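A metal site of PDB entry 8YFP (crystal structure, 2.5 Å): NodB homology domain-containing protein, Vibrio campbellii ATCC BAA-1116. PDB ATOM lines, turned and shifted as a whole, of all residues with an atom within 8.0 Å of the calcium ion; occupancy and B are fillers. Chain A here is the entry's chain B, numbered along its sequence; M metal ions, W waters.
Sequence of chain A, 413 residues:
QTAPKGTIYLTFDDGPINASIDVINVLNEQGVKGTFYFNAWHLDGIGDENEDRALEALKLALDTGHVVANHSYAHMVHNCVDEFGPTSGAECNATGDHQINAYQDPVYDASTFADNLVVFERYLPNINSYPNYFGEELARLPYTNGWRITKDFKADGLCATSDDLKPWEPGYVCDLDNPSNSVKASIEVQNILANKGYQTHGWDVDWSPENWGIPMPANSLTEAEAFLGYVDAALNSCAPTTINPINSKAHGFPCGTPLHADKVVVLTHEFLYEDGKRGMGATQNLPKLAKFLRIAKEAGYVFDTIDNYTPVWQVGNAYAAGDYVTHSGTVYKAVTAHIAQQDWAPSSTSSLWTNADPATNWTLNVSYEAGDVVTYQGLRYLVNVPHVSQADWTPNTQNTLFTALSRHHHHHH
O of Gly 197 binds the calcium ion. The calcium ion is bound by O of Gly 329 (2.2 Å). The calcium ion is bound by water W1 (2.4 Å). Water W3 binds the calcium ion (2.4 Å). The calcium ion is bound by OE2 of Glu 137 (2.4 Å). Water W2 binds the calcium ion, at 2.4 Å.
Within 4 Å of the calcium ion: Glu 137, Gly 197 and Gly 329.
The backbone carbonyl oxygen (O) of Glu 137 lies within hydrogen-bond range of the backbone NH (N) of Gln 199, at 2.8 Å.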
ATOM      1  N   PHE A 134     -38.611  15.880  29.045  1.00  0.00           N
ATOM      2  CA  PHE A 134     -37.169  16.064  29.112  1.00  0.00           C
ATOM      3  C   PHE A 134     -36.404  14.958  28.373  1.00  0.00           C
ATOM      4  O   PHE A 134     -35.281  14.609  28.731  1.00  0.00           O
ATOM      5  CB  PHE A 134     -36.704  16.177  30.569  1.00  0.00           C
ATOM      6  CG  PHE A 134     -37.018  17.496  31.194  1.00  0.00           C
ATOM      7  CD1 PHE A 134     -38.267  17.740  31.754  1.00  0.00           C
ATOM      8  CD2 PHE A 134     -36.091  18.520  31.192  1.00  0.00           C
ATOM      9  CE1 PHE A 134     -38.561  18.984  32.301  1.00  0.00           C
ATOM     10  CE2 PHE A 134     -36.382  19.751  31.735  1.00  0.00           C
ATOM     11  CZ  PHE A 134     -37.621  19.981  32.295  1.00  0.00           C
ATOM     12  N   GLU A 136     -34.791  14.940  25.659  1.00  0.00           N
ATOM     13  CA  GLU A 136     -33.508  15.358  25.082  1.00  0.00           C
ATOM     14  C   GLU A 136     -32.470  15.736  26.130  1.00  0.00           C
ATOM     15  O   GLU A 136     -31.284  15.793  25.801  1.00  0.00           O
ATOM     16  CB  GLU A 136     -33.692  16.544  24.124  1.00  0.00           C
ATOM     17  CG  GLU A 136     -34.734  16.320  23.009  1.00  0.00           C
ATOM     18  CD  GLU A 136     -34.517  17.219  21.763  1.00  0.00           C
ATOM     19  OE1 GLU A 136     -33.794  16.776  20.845  1.00  0.00           O
ATOM     20  OE2 GLU A 136     -35.040  18.349  21.708  1.00  0.00           O
ATOM     21  N   GLU A 137     -32.884  15.975  27.374  1.00  0.00           N
ATOM     22  CA  GLU A 137     -32.027  16.563  28.398  1.00  0.00           C
ATOM     23  C   GLU A 137     -31.622  15.599  29.506  1.00  0.00           C
ATOM     24  O   GLU A 137     -30.559  15.822  30.126  1.00  0.00           O
ATOM     25  CB  GLU A 137     -32.724  17.768  29.027  1.00  0.00           C
ATOM     26  CG  GLU A 137     -33.090  18.859  28.044  1.00  0.00           C
ATOM     27  CD  GLU A 137     -31.861  19.540  27.456  1.00  0.00           C
ATOM     28  OE1 GLU A 137     -31.963  20.095  26.342  1.00  0.00           O
ATOM     29  OE2 GLU A 137     -30.793  19.521  28.110  1.00  0.00           O
ATOM     30  N   LEU A 138     -32.423  14.557  29.771  1.00  0.00           N
ATOM     31  CA  LEU A 138     -32.274  13.669  30.915  1.00  0.00           C
ATOM     32  C   LEU A 138     -32.295  12.220  30.458  1.00  0.00           C
ATOM     33  O   LEU A 138     -33.236  11.791  29.786  1.00  0.00           O
ATOM     34  CB  LEU A 138     -33.414  13.874  31.929  1.00  0.00           C
ATOM     35  CG  LEU A 138     -33.537  15.189  32.683  1.00  0.00           C
ATOM     36  CD1 LEU A 138     -34.800  15.174  33.580  1.00  0.00           C
ATOM     37  CD2 LEU A 138     -32.270  15.479  33.495  1.00  0.00           C
ATOM     38  N   LEU A 193     -23.536  10.799  25.467  1.00  0.00           N
ATOM     39  CA  LEU A 193     -24.797  11.467  25.808  1.00  0.00           C
ATOM     40  C   LEU A 193     -24.567  12.821  26.465  1.00  0.00           C
ATOM     41  O   LEU A 193     -25.302  13.777  26.216  1.00  0.00           O
ATOM     42  CB  LEU A 193     -25.648  10.584  26.726  1.00  0.00           C
ATOM     43  CG  LEU A 193     -26.207   9.296  26.142  1.00  0.00           C
ATOM     44  CD1 LEU A 193     -27.070   8.590  27.194  1.00  0.00           C
ATOM     45  CD2 LEU A 193     -26.992   9.571  24.883  1.00  0.00           C
ATOM     46  N   ALA A 194     -23.537  12.912  27.321  1.00  0.00           N
ATOM     47  CA  ALA A 194     -23.266  14.194  27.962  1.00  0.00           C
ATOM     48  C   ALA A 194     -22.857  15.239  26.937  1.00  0.00           C
ATOM     49  O   ALA A 194     -23.262  16.406  27.037  1.00  0.00           O
ATOM     50  CB  ALA A 194     -22.185  14.035  29.038  1.00  0.00           C
ATOM     51  N   LYS A 196     -24.040  15.505  24.095  1.00  0.00           N
ATOM     52  CA  LYS A 196     -25.245  15.826  23.308  1.00  0.00           C
ATOM     53  C   LYS A 196     -26.186  16.661  24.190  1.00  0.00           C
ATOM     54  O   LYS A 196     -27.282  16.962  23.746  1.00  0.00           O
ATOM     55  CB  LYS A 196     -25.852  14.526  22.778  1.00  0.00           C
ATOM     56  CG  LYS A 196     -25.177  13.914  21.560  1.00  0.00           C
ATOM     57  CD  LYS A 196     -26.032  12.834  20.909  1.00  0.00           C
ATOM     58  CE  LYS A 196     -25.256  11.645  20.435  1.00  0.00           C
ATOM     59  NZ  LYS A 196     -26.105  10.573  19.886  1.00  0.00           N
ATOM     60  N   GLY A 197     -25.767  16.956  25.427  1.00  0.00           N
ATOM     61  CA  GLY A 197     -26.536  17.882  26.278  1.00  0.00           C
ATOM     62  C   GLY A 197     -27.281  17.217  27.394  1.00  0.00           C
ATOM     63  O   GLY A 197     -28.039  17.886  28.101  1.00  0.00           O
ATOM     64  N   TYR A 198     -27.052  15.934  27.550  1.00  0.00           N
ATOM     65  CA  TYR A 198     -27.800  15.183  28.566  1.00  0.00           C
ATOM     66  C   TYR A 198     -27.129  15.158  29.887  1.00  0.00           C
ATOM     67  O   TYR A 198     -25.911  15.297  29.981  1.00  0.00           O
ATOM     68  CB  TYR A 198     -27.928  13.700  28.213  1.00  0.00           C
ATOM     69  CG  TYR A 198     -28.924  13.281  27.148  1.00  0.00           C
ATOM     70  CD1 TYR A 198     -30.215  12.921  27.488  1.00  0.00           C
ATOM     71  CD2 TYR A 198     -28.548  13.213  25.821  1.00  0.00           C
ATOM     72  CE1 TYR A 198     -31.120  12.508  26.525  1.00  0.00           C
ATOM     73  CE2 TYR A 198     -29.443  12.814  24.844  1.00  0.00           C
ATOM     74  CZ  TYR A 198     -30.733  12.470  25.202  1.00  0.00           C
ATOM     75  OH  TYR A 198     -31.600  12.079  24.239  1.00  0.00           O
ATOM     76  N   GLN A 199     -27.947  15.041  30.912  1.00  0.00           N
ATOM     77  CA  GLN A 199     -27.432  14.776  32.258  1.00  0.00           C
ATOM     78  C   GLN A 199     -27.934  13.352  32.527  1.00  0.00           C
ATOM     79  O   GLN A 199     -29.029  13.039  32.073  1.00  0.00           O
ATOM     80  CB  GLN A 199     -28.021  15.764  33.264  1.00  0.00           C
ATOM     81  CG  GLN A 199     -27.179  16.961  33.657  1.00  0.00           C
ATOM     82  CD  GLN A 199     -27.870  17.753  34.737  1.00  0.00           C
ATOM     83  OE1 GLN A 199     -29.085  17.943  34.721  1.00  0.00           O
ATOM     84  NE2 GLN A 199     -27.109  18.195  35.725  1.00  0.00           N
ATOM     85  N   THR A 326     -29.368  24.840  36.606  1.00  0.00           N
ATOM     86  CA  THR A 326     -29.575  24.641  35.183  1.00  0.00           C
ATOM     87  C   THR A 326     -30.387  25.802  34.620  1.00  0.00           C
ATOM     88  O   THR A 326     -31.196  26.425  35.307  1.00  0.00           O
ATOM     89  CB  THR A 326     -30.296  23.334  34.866  1.00  0.00           C
ATOM     90  OG1 THR A 326     -31.537  23.279  35.593  1.00  0.00           O
ATOM     91  CG2 THR A 326     -29.424  22.161  35.242  1.00  0.00           C
ATOM     92  N   HIS A 327     -30.132  26.109  33.363  1.00  0.00           N
ATOM     93  CA  HIS A 327     -30.802  27.207  32.702  1.00  0.00           C
ATOM     94  C   HIS A 327     -30.932  26.811  31.245  1.00  0.00           C
ATOM     95  O   HIS A 327     -29.914  26.513  30.611  1.00  0.00           O
ATOM     96  CB  HIS A 327     -30.016  28.505  32.845  1.00  0.00           C
ATOM     97  CG  HIS A 327     -30.622  29.665  32.129  1.00  0.00           C
ATOM     98  ND1 HIS A 327     -30.254  30.019  30.852  1.00  0.00           N
ATOM     99  CD2 HIS A 327     -31.569  30.548  32.512  1.00  0.00           C
ATOM    100  CE1 HIS A 327     -30.944  31.084  30.475  1.00  0.00           C
ATOM    101  NE2 HIS A 327     -31.745  31.419  31.462  1.00  0.00           N
ATOM    102  N   SER A 328     -32.164  26.790  30.728  1.00  0.00           N
ATOM    103  CA  SER A 328     -32.397  26.306  29.380  1.00  0.00           C
ATOM    104  C   SER A 328     -31.607  25.032  29.096  1.00  0.00           C
ATOM    105  O   SER A 328     -30.979  24.932  28.039  1.00  0.00           O
ATOM    106  CB  SER A 328     -32.015  27.366  28.344  1.00  0.00           C
ATOM    107  OG  SER A 328     -32.880  28.467  28.427  1.00  0.00           O
ATOM    108  N   GLY A 329     -31.569  24.089  30.035  1.00  0.00           N
ATOM    109  CA  GLY A 329     -30.946  22.801  29.822  1.00  0.00           C
ATOM    110  C   GLY A 329     -29.471  22.716  30.133  1.00  0.00           C
ATOM    111  O   GLY A 329     -28.923  21.612  30.190  1.00  0.00           O
ATOM    112  N   THR A 330     -28.787  23.839  30.354  1.00  0.00           N
ATOM    113  CA  THR A 330     -27.358  23.839  30.582  1.00  0.00           C
ATOM    114  C   THR A 330     -27.061  24.021  32.067  1.00  0.00           C
ATOM    115  O   THR A 330     -27.792  24.726  32.774  1.00  0.00           O
ATOM    116  CB  THR A 330     -26.705  24.936  29.741  1.00  0.00           C
ATOM    117  OG1 THR A 330     -26.899  24.625  28.357  1.00  0.00           O
ATOM    118  CG2 THR A 330     -25.226  25.070  30.022  1.00  0.00           C
ATOM    119  N   VAL A 331     -25.998  23.372  32.552  1.00  0.00           N
ATOM    120  CA  VAL A 331     -25.579  23.477  33.947  1.00  0.00           C
ATOM    121  C   VAL A 331     -24.597  24.627  34.080  1.00  0.00           C
ATOM    122  O   VAL A 331     -23.659  24.741  33.293  1.00  0.00           O
ATOM    123  CB  VAL A 331     -24.931  22.153  34.428  1.00  0.00           C
ATOM    124  CG1 VAL A 331     -24.360  22.322  35.819  1.00  0.00           C
ATOM    125  CG2 VAL A 331     -25.971  21.030  34.425  1.00  0.00           C
ATOM    126  N   ASP A 357     -21.518  22.063  32.430  1.00  0.00           N
ATOM    127  CA  ASP A 357     -22.066  20.835  31.874  1.00  0.00           C
ATOM    128  C   ASP A 357     -21.073  19.687  32.031  1.00  0.00           C
ATOM    129  O   ASP A 357     -19.863  19.879  31.942  1.00  0.00           O
ATOM    130  CB  ASP A 357     -22.409  21.008  30.399  1.00  0.00           C
ATOM    131  CG  ASP A 357     -23.843  21.461  30.183  1.00  0.00           C
ATOM    132  OD1 ASP A 357     -24.138  22.016  29.092  1.00  0.00           O
ATOM    133  OD2 ASP A 357     -24.686  21.271  31.090  1.00  0.00           O
ATOM    134  N   PRO A 358     -21.573  18.465  32.251  1.00  0.00           N
ATOM    135  CA  PRO A 358     -20.674  17.308  32.330  1.00  0.00           C
ATOM    136  C   PRO A 358     -20.091  16.861  31.000  1.00  0.00           C
ATOM    137  O   PRO A 358     -19.476  15.782  30.957  1.00  0.00           O
ATOM    138  CB  PRO A 358     -21.592  16.219  32.917  1.00  0.00           C
ATOM    139  CG  PRO A 358     -22.970  16.581  32.438  1.00  0.00           C
ATOM    140  CD  PRO A 358     -22.992  18.103  32.401  1.00  0.00           C
HETATM  141 CA    CA M   1     -28.603  19.779  29.025  1.00  0.00          CA
HETATM  142  O   HOH W   1     -26.568  19.327  30.137  1.00  0.00           O
HETATM  143  O   HOH W   2     -29.523  18.324  30.746  1.00  0.00           O
HETATM  144  O   HOH W   3     -27.042  21.016  27.723  1.00  0.00           O
